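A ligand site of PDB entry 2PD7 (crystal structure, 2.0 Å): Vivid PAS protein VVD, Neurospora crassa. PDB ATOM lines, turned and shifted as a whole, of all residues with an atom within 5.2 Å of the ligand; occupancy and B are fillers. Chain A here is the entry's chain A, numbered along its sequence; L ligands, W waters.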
ATOM      1  N   ILE A  39      23.145 -24.284  23.240  1.00  0.00           N
ATOM      2  CA  ILE A  39      21.950 -24.416  22.444  1.00  0.00           C
ATOM      3  C   ILE A  39      22.178 -25.485  21.390  1.00  0.00           C
ATOM      4  O   ILE A  39      23.312 -25.786  21.009  1.00  0.00           O
ATOM      5  CB  ILE A  39      21.548 -23.109  21.746  1.00  0.00           C
ATOM      6  CG1 ILE A  39      22.661 -22.627  20.815  1.00  0.00           C
ATOM      7  CG2 ILE A  39      21.214 -22.043  22.791  1.00  0.00           C
ATOM      8  CD1 ILE A  39      22.243 -21.418  20.013  1.00  0.00           C
ATOM      9  N   LEU A  40      21.075 -26.095  20.976  1.00  0.00           N
ATOM     10  CA  LEU A  40      21.114 -27.125  19.959  1.00  0.00           C
ATOM     11  C   LEU A  40      20.237 -26.629  18.801  1.00  0.00           C
ATOM     12  O   LEU A  40      19.090 -26.214  19.020  1.00  0.00           O
ATOM     13  CB  LEU A  40      20.584 -28.457  20.525  1.00  0.00           C
ATOM     14  CG  LEU A  40      20.758 -29.671  19.595  1.00  0.00           C
ATOM     15  CD1 LEU A  40      22.212 -30.174  19.660  1.00  0.00           C
ATOM     16  CD2 LEU A  40      19.772 -30.788  19.990  1.00  0.00           C
ATOM     17  N   CYS A  41      20.783 -26.627  17.575  1.00  0.00           N
ATOM     18  CA  CYS A  41      20.048 -26.184  16.389  1.00  0.00           C
ATOM     19  C   CYS A  41      19.876 -27.368  15.453  1.00  0.00           C
ATOM     20  O   CYS A  41      20.704 -28.287  15.455  1.00  0.00           O
ATOM     21  CB  CYS A  41      20.794 -25.069  15.663  1.00  0.00           C
ATOM     22  SG  CYS A  41      21.053 -23.556  16.634  1.00  0.00           S
ATOM     23  N   ASP A  47      16.529 -22.958   7.789  1.00  0.00           N
ATOM     24  CA  ASP A  47      17.293 -21.892   8.432  1.00  0.00           C
ATOM     25  C   ASP A  47      17.916 -22.251   9.789  1.00  0.00           C
ATOM     26  O   ASP A  47      18.079 -21.382  10.658  1.00  0.00           O
ATOM     27  CB  ASP A  47      16.448 -20.605   8.559  1.00  0.00           C
ATOM     28  CG  ASP A  47      17.317 -19.345   8.598  1.00  0.00           C
ATOM     29  OD1 ASP A  47      18.449 -19.386   8.083  1.00  0.00           O
ATOM     30  OD2 ASP A  47      16.857 -18.317   9.122  1.00  0.00           O
ATOM     31  N   THR A  48      18.251 -23.521   9.980  1.00  0.00           N
ATOM     32  CA  THR A  48      18.930 -24.013  11.184  1.00  0.00           C
ATOM     33  C   THR A  48      18.392 -23.441  12.489  1.00  0.00           C
ATOM     34  O   THR A  48      19.097 -22.744  13.218  1.00  0.00           O
ATOM     35  CB  THR A  48      20.438 -23.696  11.064  1.00  0.00           C
ATOM     36  OG1 THR A  48      20.849 -23.942   9.708  1.00  0.00           O
ATOM     37  CG2 THR A  48      21.257 -24.590  11.999  1.00  0.00           C
ATOM     38  N   PHE A  57      21.860 -20.133  28.985  1.00  0.00           N
ATOM     39  CA  PHE A  57      21.803 -19.353  27.747  1.00  0.00           C
ATOM     40  C   PHE A  57      20.731 -18.278  27.864  1.00  0.00           C
ATOM     41  O   PHE A  57      20.969 -17.110  27.590  1.00  0.00           O
ATOM     42  CB  PHE A  57      21.451 -20.241  26.540  1.00  0.00           C
ATOM     43  CG  PHE A  57      21.219 -19.473  25.251  1.00  0.00           C
ATOM     44  CD1 PHE A  57      22.295 -19.054  24.476  1.00  0.00           C
ATOM     45  CD2 PHE A  57      19.925 -19.199  24.809  1.00  0.00           C
ATOM     46  CE1 PHE A  57      22.094 -18.370  23.274  1.00  0.00           C
ATOM     47  CE2 PHE A  57      19.707 -18.523  23.621  1.00  0.00           C
ATOM     48  CZ  PHE A  57      20.798 -18.109  22.839  1.00  0.00           C
ATOM     49  N   ASN A  72      16.581 -18.718  14.149  1.00  0.00           N
ATOM     50  CA  ASN A  72      17.979 -18.902  13.831  1.00  0.00           C
ATOM     51  C   ASN A  72      18.668 -17.973  14.838  1.00  0.00           C
ATOM     52  O   ASN A  72      18.222 -16.856  15.049  1.00  0.00           O
ATOM     53  CB  ASN A  72      18.281 -18.467  12.406  1.00  0.00           C
ATOM     54  CG  ASN A  72      19.751 -18.596  12.056  1.00  0.00           C
ATOM     55  OD1 ASN A  72      20.553 -17.728  12.384  1.00  0.00           O
ATOM     56  ND2 ASN A  72      20.114 -19.694  11.404  1.00  0.00           N
ATOM     57  N   CYS A  73      19.737 -18.435  15.457  1.00  0.00           N
ATOM     58  CA  CYS A  73      20.425 -17.630  16.459  1.00  0.00           C
ATOM     59  C   CYS A  73      21.045 -16.289  16.010  1.00  0.00           C
ATOM     60  O   CYS A  73      21.586 -15.567  16.827  1.00  0.00           O
ATOM     61  CB  CYS A  73      21.487 -18.501  17.162  1.00  0.00           C
ATOM     62  SG  CYS A  73      21.878 -18.011  18.867  1.00  0.00           S
ATOM     63  N   ARG A  74      20.936 -15.942  14.719  1.00  0.00           N
ATOM     64  CA  ARG A  74      21.523 -14.689  14.252  1.00  0.00           C
ATOM     65  C   ARG A  74      20.837 -13.458  14.838  1.00  0.00           C
ATOM     66  O   ARG A  74      21.401 -12.352  14.798  1.00  0.00           O
ATOM     67  CB  ARG A  74      21.535 -14.618  12.711  1.00  0.00           C
ATOM     68  CG  ARG A  74      20.188 -14.340  12.038  1.00  0.00           C
ATOM     69  CD  ARG A  74      20.355 -14.045  10.516  1.00  0.00           C
ATOM     70  NE  ARG A  74      20.732 -15.218   9.735  1.00  0.00           N
ATOM     71  CZ  ARG A  74      19.900 -16.200   9.415  1.00  0.00           C
ATOM     72  NH1 ARG A  74      20.338 -17.223   8.693  1.00  0.00           N
ATOM     73  NH2 ARG A  74      18.627 -16.167   9.804  1.00  0.00           N
ATOM     74  N   LEU A  76      20.608 -12.513  17.701  1.00  0.00           N
ATOM     75  CA  LEU A  76      21.426 -11.919  18.757  1.00  0.00           C
ATOM     76  C   LEU A  76      22.382 -10.872  18.206  1.00  0.00           C
ATOM     77  O   LEU A  76      22.914 -10.055  18.959  1.00  0.00           O
ATOM     78  CB  LEU A  76      22.251 -12.980  19.487  1.00  0.00           C
ATOM     79  CG  LEU A  76      21.507 -13.945  20.405  1.00  0.00           C
ATOM     80  CD1 LEU A  76      22.463 -15.058  20.835  1.00  0.00           C
ATOM     81  CD2 LEU A  76      20.951 -13.211  21.618  1.00  0.00           C
ATOM     82  N   GLN A  77      22.590 -10.896  16.904  1.00  0.00           N
ATOM     83  CA  GLN A  77      23.512  -9.966  16.270  1.00  0.00           C
ATOM     84  C   GLN A  77      23.016  -8.520  16.204  1.00  0.00           C
ATOM     85  O   GLN A  77      23.767  -7.644  15.775  1.00  0.00           O
ATOM     86  CB  GLN A  77      23.878 -10.492  14.888  1.00  0.00           C
ATOM     87  CG  GLN A  77      24.809 -11.705  14.964  1.00  0.00           C
ATOM     88  CD  GLN A  77      24.814 -12.569  13.716  1.00  0.00           C
ATOM     89  OE1 GLN A  77      24.601 -12.076  12.607  1.00  0.00           O
ATOM     90  NE2 GLN A  77      25.101 -13.849  13.895  1.00  0.00           N
ATOM     91  N   LYS A  84      17.756  -9.758   9.234  1.00  0.00           N
ATOM     92  CA  LYS A  84      17.362 -10.377   8.002  1.00  0.00           C
ATOM     93  C   LYS A  84      18.456 -11.267   7.425  1.00  0.00           C
ATOM     94  O   LYS A  84      19.620 -10.906   7.439  1.00  0.00           O
ATOM     95  CB  LYS A  84      17.022  -9.262   7.035  1.00  0.00           C
ATOM     96  CG  LYS A  84      17.935  -8.013   7.177  1.00  0.00           C
ATOM     97  CD  LYS A  84      17.392  -6.889   8.101  1.00  0.00           C
ATOM     98  CE  LYS A  84      17.942  -6.953   9.520  1.00  0.00           C
ATOM     99  NZ  LYS A  84      17.687  -5.702  10.273  1.00  0.00           N
ATOM    100  N   PRO A  85      18.082 -12.448   6.891  1.00  0.00           N
ATOM    101  CA  PRO A  85      19.072 -13.351   6.302  1.00  0.00           C
ATOM    102  C   PRO A  85      19.894 -12.620   5.242  1.00  0.00           C
ATOM    103  O   PRO A  85      19.381 -11.764   4.506  1.00  0.00           O
ATOM    104  CB  PRO A  85      18.208 -14.450   5.699  1.00  0.00           C
ATOM    105  CG  PRO A  85      17.031 -14.493   6.617  1.00  0.00           C
ATOM    106  CD  PRO A  85      16.726 -13.039   6.842  1.00  0.00           C
ATOM    107  N   LYS A  86      21.174 -12.970   5.173  1.00  0.00           N
ATOM    108  CA  LYS A  86      22.150 -12.403   4.225  1.00  0.00           C
ATOM    109  C   LYS A  86      22.308 -10.888   4.205  1.00  0.00           C
ATOM    110  O   LYS A  86      22.989 -10.347   3.332  1.00  0.00           O
ATOM    111  CB  LYS A  86      21.878 -12.900   2.800  1.00  0.00           C
ATOM    112  CG  LYS A  86      20.660 -13.797   2.622  1.00  0.00           C
ATOM    113  CD  LYS A  86      21.033 -15.194   2.151  1.00  0.00           C
ATOM    114  CE  LYS A  86      22.019 -15.873   3.106  1.00  0.00           C
ATOM    115  NZ  LYS A  86      21.644 -15.678   4.550  1.00  0.00           N
ATOM    116  N   SER A  87      21.694 -10.184   5.139  1.00  0.00           N
ATOM    117  CA  SER A  87      21.813  -8.722   5.177  1.00  0.00           C
ATOM    118  C   SER A  87      23.181  -8.319   5.688  1.00  0.00           C
ATOM    119  O   SER A  87      23.844  -9.097   6.384  1.00  0.00           O
ATOM    120  CB  SER A  87      20.768  -8.145   6.103  1.00  0.00           C
ATOM    121  OG  SER A  87      21.009  -8.621   7.418  1.00  0.00           O
ATOM    122  N   THR A  88      23.597  -7.097   5.367  1.00  0.00           N
ATOM    123  CA  THR A  88      24.887  -6.596   5.821  1.00  0.00           C
ATOM    124  C   THR A  88      24.698  -6.001   7.227  1.00  0.00           C
ATOM    125  O   THR A  88      24.066  -4.961   7.385  1.00  0.00           O
ATOM    126  CB  THR A  88      25.443  -5.495   4.881  1.00  0.00           C
ATOM    127  OG1 THR A  88      25.633  -6.027   3.573  1.00  0.00           O
ATOM    128  CG2 THR A  88      26.762  -4.971   5.410  1.00  0.00           C
ATOM    129  N   ARG A  89      25.244  -6.671   8.223  1.00  0.00           N
ATOM    130  CA  ARG A  89      25.129  -6.222   9.614  1.00  0.00           C
ATOM    131  C   ARG A  89      25.812  -4.885   9.870  1.00  0.00           C
ATOM    132  O   ARG A  89      26.878  -4.604   9.340  1.00  0.00           O
ATOM    133  CB  ARG A  89      25.700  -7.265  10.561  1.00  0.00           C
ATOM    134  CG  ARG A  89      24.716  -8.357  10.942  1.00  0.00           C
ATOM    135  CD  ARG A  89      24.257  -9.182   9.756  1.00  0.00           C
ATOM    136  NE  ARG A  89      24.100 -10.575  10.150  1.00  0.00           N
ATOM    137  CZ  ARG A  89      23.817 -11.578   9.326  1.00  0.00           C
ATOM    138  NH1 ARG A  89      23.719 -12.806   9.805  1.00  0.00           N
ATOM    139  NH2 ARG A  89      23.626 -11.346   8.035  1.00  0.00           N
ATOM    140  N   SER A  94      31.555  -8.565   9.120  1.00  0.00           N
ATOM    141  CA  SER A  94      31.064  -9.368   7.996  1.00  0.00           C
ATOM    142  C   SER A  94      31.884 -10.630   7.766  1.00  0.00           C
ATOM    143  O   SER A  94      31.337 -11.667   7.398  1.00  0.00           O
ATOM    144  CB  SER A  94      31.050  -8.527   6.715  1.00  0.00           C
ATOM    145  OG  SER A  94      30.081  -7.496   6.815  1.00  0.00           O
ATOM    146  N   ILE A  97      30.932 -13.301  10.618  1.00  0.00           N
ATOM    147  CA  ILE A  97      29.705 -14.030  10.376  1.00  0.00           C
ATOM    148  C   ILE A  97      29.740 -14.933   9.150  1.00  0.00           C
ATOM    149  O   ILE A  97      28.977 -15.894   9.066  1.00  0.00           O
ATOM    150  CB  ILE A  97      28.484 -13.060  10.368  1.00  0.00           C
ATOM    151  CG1 ILE A  97      28.786 -11.815   9.550  1.00  0.00           C
ATOM    152  CG2 ILE A  97      28.165 -12.617  11.798  1.00  0.00           C
ATOM    153  CD1 ILE A  97      27.823 -10.666   9.845  1.00  0.00           C
ATOM    154  N   ASN A  98      30.622 -14.649   8.189  1.00  0.00           N
ATOM    155  CA  ASN A  98      30.684 -15.525   7.016  1.00  0.00           C
ATOM    156  C   ASN A  98      31.491 -16.767   7.380  1.00  0.00           C
ATOM    157  O   ASN A  98      31.297 -17.829   6.798  1.00  0.00           O
ATOM    158  CB  ASN A  98      31.328 -14.821   5.821  1.00  0.00           C
ATOM    159  CG  ASN A  98      31.317 -15.676   4.557  1.00  0.00           C
ATOM    160  OD1 ASN A  98      30.265 -16.115   4.094  1.00  0.00           O
ATOM    161  ND2 ASN A  98      32.498 -15.917   4.002  1.00  0.00           N
ATOM    162  N   MET A 100      31.261 -18.236  10.173  1.00  0.00           N
ATOM    163  CA  MET A 100      30.300 -19.099  10.846  1.00  0.00           C
ATOM    164  C   MET A 100      29.425 -19.823   9.839  1.00  0.00           C
ATOM    165  O   MET A 100      29.221 -21.027   9.925  1.00  0.00           O
ATOM    166  CB  MET A 100      29.398 -18.286  11.767  1.00  0.00           C
ATOM    167  CG  MET A 100      30.094 -17.679  12.968  1.00  0.00           C
ATOM    168  SD  MET A 100      28.914 -16.900  14.127  1.00  0.00           S
ATOM    169  CE  MET A 100      28.787 -15.270  13.469  1.00  0.00           C
ATOM    170  N   ARG A 101      28.890 -19.064   8.886  1.00  0.00           N
ATOM    171  CA  ARG A 101      28.024 -19.627   7.876  1.00  0.00           C
ATOM    172  C   ARG A 101      28.686 -20.775   7.115  1.00  0.00           C
ATOM    173  O   ARG A 101      28.111 -21.840   6.895  1.00  0.00           O
ATOM    174  CB  ARG A 101      27.603 -18.523   6.918  1.00  0.00           C
ATOM    175  CG  ARG A 101      26.755 -18.999   5.763  1.00  0.00           C
ATOM    176  CD  ARG A 101      26.209 -17.833   4.964  1.00  0.00           C
ATOM    177  NE  ARG A 101      26.110 -18.206   3.557  1.00  0.00           N
ATOM    178  CZ  ARG A 101      27.165 -18.422   2.779  1.00  0.00           C
ATOM    179  NH1 ARG A 101      28.389 -18.291   3.261  1.00  0.00           N
ATOM    180  NH2 ARG A 101      26.992 -18.812   1.516  1.00  0.00           N
ATOM    181  N   ILE A 104      29.410 -23.937   9.431  1.00  0.00           N
ATOM    182  CA  ILE A 104      28.196 -24.705   9.596  1.00  0.00           C
ATOM    183  C   ILE A 104      27.855 -25.448   8.314  1.00  0.00           C
ATOM    184  O   ILE A 104      27.539 -26.638   8.349  1.00  0.00           O
ATOM    185  CB  ILE A 104      27.043 -23.772   9.995  1.00  0.00           C
ATOM    186  CG1 ILE A 104      27.366 -23.144  11.357  1.00  0.00           C
ATOM    187  CG2 ILE A 104      25.738 -24.549  10.043  1.00  0.00           C
ATOM    188  CD1 ILE A 104      26.665 -21.857  11.608  1.00  0.00           C
ATOM    189  N   VAL A 114      32.179 -12.913  18.529  1.00  0.00           N
ATOM    190  CA  VAL A 114      31.237 -12.125  17.759  1.00  0.00           C
ATOM    191  C   VAL A 114      30.444 -11.198  18.669  1.00  0.00           C
ATOM    192  O   VAL A 114      30.113 -11.566  19.789  1.00  0.00           O
ATOM    193  CB  VAL A 114      30.277 -13.062  16.967  1.00  0.00           C
ATOM    194  CG1 VAL A 114      29.498 -13.940  17.932  1.00  0.00           C
ATOM    195  CG2 VAL A 114      29.340 -12.237  16.076  1.00  0.00           C
ATOM    196  N   VAL A 115      30.174  -9.991  18.205  1.00  0.00           N
ATOM    197  CA  VAL A 115      29.394  -9.048  19.002  1.00  0.00           C
ATOM    198  C   VAL A 115      27.915  -9.468  18.945  1.00  0.00           C
ATOM    199  O   VAL A 115      27.387  -9.721  17.863  1.00  0.00           O
ATOM    200  CB  VAL A 115      29.554  -7.596  18.482  1.00  0.00           C
ATOM    201  CG1 VAL A 115      28.712  -6.655  19.321  1.00  0.00           C
ATOM    202  CG2 VAL A 115      31.012  -7.164  18.557  1.00  0.00           C
ATOM    203  N   ASN A 116      27.289  -9.562  20.111  1.00  0.00           N
ATOM    204  CA  ASN A 116      25.871  -9.927  20.219  1.00  0.00           C
ATOM    205  C   ASN A 116      25.253  -8.907  21.148  1.00  0.00           C
ATOM    206  O   ASN A 116      25.961  -8.084  21.727  1.00  0.00           O
ATOM    207  CB  ASN A 116      25.679 -11.324  20.843  1.00  0.00           C
ATOM    208  CG  ASN A 116      25.870 -12.457  19.844  1.00  0.00           C
ATOM    209  OD1 ASN A 116      25.857 -13.635  20.238  1.00  0.00           O
ATOM    210  ND2 ASN A 116      26.043 -12.127  18.570  1.00  0.00           N
ATOM    211  N   ASN A 126      30.577 -12.340  22.445  1.00  0.00           N
ATOM    212  CA  ASN A 126      30.218 -13.727  22.670  1.00  0.00           C
ATOM    213  C   ASN A 126      31.328 -14.632  22.184  1.00  0.00           C
ATOM    214  O   ASN A 126      31.617 -14.649  20.996  1.00  0.00           O
ATOM    215  CB  ASN A 126      28.909 -14.056  21.926  1.00  0.00           C
ATOM    216  CG  ASN A 126      28.387 -15.441  22.244  1.00  0.00           C
ATOM    217  OD1 ASN A 126      29.077 -16.267  22.846  1.00  0.00           O
ATOM    218  ND2 ASN A 126      27.137 -15.711  21.843  1.00  0.00           N
ATOM    219  N   LEU A 128      32.051 -17.774  21.070  1.00  0.00           N
ATOM    220  CA  LEU A 128      31.255 -18.859  20.532  1.00  0.00           C
ATOM    221  C   LEU A 128      31.951 -20.049  19.861  1.00  0.00           C
ATOM    222  O   LEU A 128      32.778 -19.888  18.964  1.00  0.00           O
ATOM    223  CB  LEU A 128      30.250 -18.253  19.546  1.00  0.00           C
ATOM    224  CG  LEU A 128      29.358 -19.159  18.690  1.00  0.00           C
ATOM    225  CD1 LEU A 128      28.270 -19.729  19.570  1.00  0.00           C
ATOM    226  CD2 LEU A 128      28.747 -18.353  17.519  1.00  0.00           C
ATOM    227  N   MET A 130      30.981 -23.776  17.961  1.00  0.00           N
ATOM    228  CA  MET A 130      29.901 -24.560  17.358  1.00  0.00           C
ATOM    229  C   MET A 130      30.438 -25.908  16.899  1.00  0.00           C
ATOM    230  O   MET A 130      31.395 -25.980  16.116  1.00  0.00           O
ATOM    231  CB  MET A 130      29.294 -23.791  16.166  1.00  0.00           C
ATOM    232  CG  MET A 130      28.649 -22.465  16.552  1.00  0.00           C
ATOM    233  SD  MET A 130      28.037 -21.513  15.135  1.00  0.00           S
ATOM    234  CE  MET A 130      29.571 -20.883  14.450  1.00  0.00           C
ATOM    235  N   SER A 143      23.711 -29.164  15.642  1.00  0.00           N
ATOM    236  CA  SER A 143      24.924 -28.423  15.961  1.00  0.00           C
ATOM    237  C   SER A 143      24.746 -27.887  17.364  1.00  0.00           C
ATOM    238  O   SER A 143      23.708 -27.307  17.678  1.00  0.00           O
ATOM    239  CB  SER A 143      25.120 -27.251  15.011  1.00  0.00           C
ATOM    240  OG  SER A 143      26.277 -26.502  15.376  1.00  0.00           O
ATOM    241  N   MET A 144      25.758 -28.074  18.212  1.00  0.00           N
ATOM    242  CA  MET A 144      25.694 -27.562  19.564  1.00  0.00           C
ATOM    243  C   MET A 144      26.587 -26.340  19.712  1.00  0.00           C
ATOM    244  O   MET A 144      27.783 -26.370  19.373  1.00  0.00           O
ATOM    245  CB  MET A 144      26.110 -28.618  20.591  1.00  0.00           C
ATOM    246  CG  MET A 144      25.787 -28.184  22.006  1.00  0.00           C
ATOM    247  SD  MET A 144      25.814 -29.498  23.202  1.00  0.00           S
ATOM    248  CE  MET A 144      24.203 -30.261  22.965  1.00  0.00           C
ATOM    249  N   GLY A 145      25.988 -25.267  20.207  1.00  0.00           N
ATOM    250  CA  GLY A 145      26.710 -24.036  20.413  1.00  0.00           C
ATOM    251  C   GLY A 145      26.951 -23.842  21.889  1.00  0.00           C
ATOM    252  O   GLY A 145      26.102 -24.163  22.718  1.00  0.00           O
ATOM    253  N   GLN A 147      28.079 -20.758  24.281  1.00  0.00           N
ATOM    254  CA  GLN A 147      28.272 -19.311  24.333  1.00  0.00           C
ATOM    255  C   GLN A 147      28.927 -18.850  25.630  1.00  0.00           C
ATOM    256  O   GLN A 147      28.520 -19.272  26.715  1.00  0.00           O
ATOM    257  CB  GLN A 147      26.937 -18.568  24.164  1.00  0.00           C
ATOM    258  CG  GLN A 147      26.312 -18.676  22.775  1.00  0.00           C
ATOM    259  CD  GLN A 147      25.537 -19.971  22.561  1.00  0.00           C
ATOM    260  OE1 GLN A 147      25.332 -20.752  23.493  1.00  0.00           O
ATOM    261  NE2 GLN A 147      25.105 -20.212  21.331  1.00  0.00           N
HETATM  262  P1  LIG L   1      24.306 -14.553   6.122  1.00  0.00           P
HETATM  263  O1  LIG L   1      22.959 -14.089   6.524  1.00  0.00           O
HETATM  264  O2  LIG L   1      24.462 -15.157   4.768  1.00  0.00           O
HETATM  265  O3  LIG L   1      25.295 -13.323   6.300  1.00  0.00           O
HETATM  266  C1  LIG L   1      26.683 -13.363   5.978  1.00  0.00           C
HETATM  267  C2  LIG L   1      27.287 -11.952   6.137  1.00  0.00           C
HETATM  268  O4  LIG L   1      28.691 -12.132   5.856  1.00  0.00           O
HETATM  269  C3  LIG L   1      26.768 -10.897   5.146  1.00  0.00           C
HETATM  270  O5  LIG L   1      26.295  -9.782   5.839  1.00  0.00           O
HETATM  271  C4  LIG L   1      27.936 -10.520   4.227  1.00  0.00           C
HETATM  272  O6  LIG L   1      28.235  -9.145   4.041  1.00  0.00           O
HETATM  273  C5  LIG L   1      29.132 -11.314   4.727  1.00  0.00           C
HETATM  274  N1  LIG L   1      29.647 -12.255   3.703  1.00  0.00           N
HETATM  275  C6  LIG L   1      29.086 -13.440   3.317  1.00  0.00           C
HETATM  276  N2  LIG L   1      29.736 -14.082   2.382  1.00  0.00           N
HETATM  277  C7  LIG L   1      30.803 -13.276   2.114  1.00  0.00           C
HETATM  278  C8  LIG L   1      31.861 -13.440   1.186  1.00  0.00           C
HETATM  279  N3  LIG L   1      31.914 -14.537   0.411  1.00  0.00           N
HETATM  280  N4  LIG L   1      32.822 -12.466   1.095  1.00  0.00           N
HETATM  281  C9  LIG L   1      32.720 -11.384   1.935  1.00  0.00           C
HETATM  282  N5  LIG L   1      31.740 -11.114   2.849  1.00  0.00           N
HETATM  283  C10 LIG L   1      30.792 -12.146   2.882  1.00  0.00           C
HETATM  284  N6  LIG L   1      25.410 -16.416  16.038  1.00  0.00           N
HETATM  285  C11 LIG L   1      25.496 -15.419  16.960  1.00  0.00           C
HETATM  286  O7  LIG L   1      25.637 -14.225  16.645  1.00  0.00           O
HETATM  287  N7  LIG L   1      25.429 -15.739  18.313  1.00  0.00           N
HETATM  288  C12 LIG L   1      25.267 -17.039  18.812  1.00  0.00           C
HETATM  289  O8  LIG L   1      25.227 -17.230  20.035  1.00  0.00           O
HETATM  290  C13 LIG L   1      25.172 -18.060  17.845  1.00  0.00           C
HETATM  291  N8  LIG L   1      25.012 -19.399  18.276  1.00  0.00           N
HETATM  292  C14 LIG L   1      24.918 -20.386  17.297  1.00  0.00           C
HETATM  293  C15 LIG L   1      24.754 -21.751  17.697  1.00  0.00           C
HETATM  294  C16 LIG L   1      24.638 -22.788  16.784  1.00  0.00           C
HETATM  295  C17 LIG L   1      24.479 -24.222  17.321  1.00  0.00           C
HETATM  296  C18 LIG L   1      24.668 -22.514  15.403  1.00  0.00           C
HETATM  297  C19 LIG L   1      24.542 -23.588  14.351  1.00  0.00           C
HETATM  298  C20 LIG L   1      24.837 -21.140  14.963  1.00  0.00           C
HETATM  299  C21 LIG L   1      24.970 -20.078  15.880  1.00  0.00           C
HETATM  300  N9  LIG L   1      25.151 -18.688  15.483  1.00  0.00           N
HETATM  301  C22 LIG L   1      25.246 -17.702  16.462  1.00  0.00           C
HETATM  302  C23 LIG L   1      25.272 -18.275  14.047  1.00  0.00           C
HETATM  303  C24 LIG L   1      24.030 -17.882  13.248  1.00  0.00           C
HETATM  304  O9  LIG L   1      22.935 -18.721  13.641  1.00  0.00           O
HETATM  305  C25 LIG L   1      24.385 -18.013  11.727  1.00  0.00           C
HETATM  306  O10 LIG L   1      24.745 -19.357  11.490  1.00  0.00           O
HETATM  307  C26 LIG L   1      25.584 -17.105  11.274  1.00  0.00           C
HETATM  308  O11 LIG L   1      25.278 -15.736  11.505  1.00  0.00           O
HETATM  309  C27 LIG L   1      25.970 -17.291   9.803  1.00  0.00           C
HETATM  310  O12 LIG L   1      24.829 -17.569   8.962  1.00  0.00           O
HETATM  311  P2  LIG L   1      23.930 -16.423   8.342  1.00  0.00           P
HETATM  312  O13 LIG L   1      22.741 -17.106   7.826  1.00  0.00           O
HETATM  313  O14 LIG L   1      23.697 -15.358   9.360  1.00  0.00           O
HETATM  314  O15 LIG L   1      24.731 -15.739   7.124  1.00  0.00           O
HETATM  315  O   HOH W   1      25.234  -8.761   2.798  1.00  0.00           O
HETATM  316  O   HOH W   2      21.080 -21.147  14.587  1.00  0.00           O
HETATM  317  O   HOH W   3      27.600  -8.360   7.947  1.00  0.00           O
HETATM  318  O   HOH W   4      33.779 -16.649   0.615  1.00  0.00           O
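Water W3 lies within hydrogen-bond range of O5 of the ligand (2.9 Å), OG of Ser 94 (2.9 Å) and N of Arg 89 (2.9 Å). Water W2 lies within hydrogen-bond range of the backbone carbonyl oxygen (O) of Thr 48, the backbone NH (N) of Cys 73, the side-chain sulfur (SG) of Cys 41 and an oxygen (O9) of the ligand. Water W1 lies within hydrogen-bond range of O of Lys 86 (2.8 Å), OG1 of Thr 88 (2.9 Å) and O6 of the ligand (3.3 Å).
An oxygen (O13) of the ligand is in salt-bridge range of the guanidinium group of Arg 74. O1 of the ligand is in hydrogen-bond range of N of Lys 86, at 2.5 Å. The backbone carbonyl oxygen of Ser 87 sits at hydrogen-bond distance from an oxygen (O5) of the ligand (2.6 Å). An oxygen (O14) of the ligand lies within salt-bridge range of the guanidinium group (NH1) of Arg 89, 2.6 Å away. An oxygen (O7) of the ligand sits at hydrogen-bond distance from the side-chain amide nitrogen (ND2) of Asn 116, 2.9 Å away. An oxygen (O9) of the ligand lies within hydrogen-bond range of the side-chain amide oxygen (OD1) of Asn 72, 2.9 Å away. A nitrogen (N2) of the ligand sits close to the side-chain amide oxygen (OD1) of Asn 98, at 2.7 Å. The guanidinium group (NE) of Arg 101 is in salt-bridge range of an oxygen (O2) of the ligand (3.7 Å). The side-chain sulfur of Cys 73 sits close to a nitrogen (N8) of the ligand (3.5 Å). A nitrogen (N8) of the ligand is in hydrogen-bond range of the side-chain amide nitrogen (NE2) of Gln 147. The side-chain amide nitrogen (NE2) of Gln 77 lies within hydrogen-bond range of an oxygen (O7) of the ligand (2.8 Å). An oxygen (O8) of the ligand sits at hydrogen-bond distance from the side-chain amide nitrogen (ND2) of Asn 126 (3.0 Å). An oxygen (O1) of the ligand lies within salt-bridge range of the side-chain amino group (NZ) of Lys 86.
The side-chain amide oxygen (OD1) of Asn 98 sits at hydrogen-bond distance from the guanidinium group (NH1) of Arg 101 (3.0 Å). The side-chain amide oxygen of Gln 77 sits at hydrogen-bond distance from the guanidinium group of Arg 89 (2.9 Å). O of Lys 84 sits at hydrogen-bond distance from OG of Ser 87, 2.7 Å away. The backbone carbonyl oxygen (O) of Ser 143 lies within hydrogen-bond range of the backbone NH (N) of Cys 41 (3.0 Å). N of Arg 74 is in hydrogen-bond range of OD1 of Asn 72, at 3.0 Å. The side-chain amide nitrogen (ND2) of Asn 72 lies within hydrogen-bond range of the backbone carbonyl oxygen (O) of Asp 47, 2.7 Å away. OD2 of Asp 47 is in salt-bridge range of NH2 of Arg 74, at 2.9 Å. The side-chain amide oxygen (OD1) of Asn 116 lies within hydrogen-bond range of the side-chain amide nitrogen (ND2) of Asn 126, at 2.9 Å.
O4 of the ligand lies close to O of Ser 94, at 3.1 Å. Residues that only touch the ligand: Ile 104, Ser 143, Met 130, Ile 97, Gly 145, Ile 39, Thr 88, Leu 128, Cys 41, Leu 76, Pro 85, Met 144 and Met 100. Hydrophobic or aromatic side chains that line the ligand: Ile 39, Leu 76, Ile 97, Met 100, Ile 104, Leu 128 and Met 130. 26 residues have an atom within 4 Å of the ligand: Ile 39, Cys 41, Asn 72, Cys 73, Arg 74, Leu 76, Gln 77, Pro 85, Lys 86, Ser 87, Thr 88, Arg 89, Ser 94, Ile 97, Asn 98, Met 100, Arg 101, Ile 104, Asn 116, Asn 126, Leu 128, Met 130, Ser 143, Met 144, Gly 145 and Gln 147. Along chain A the residues within 4 Å of the ligand span positions 39 to 147.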
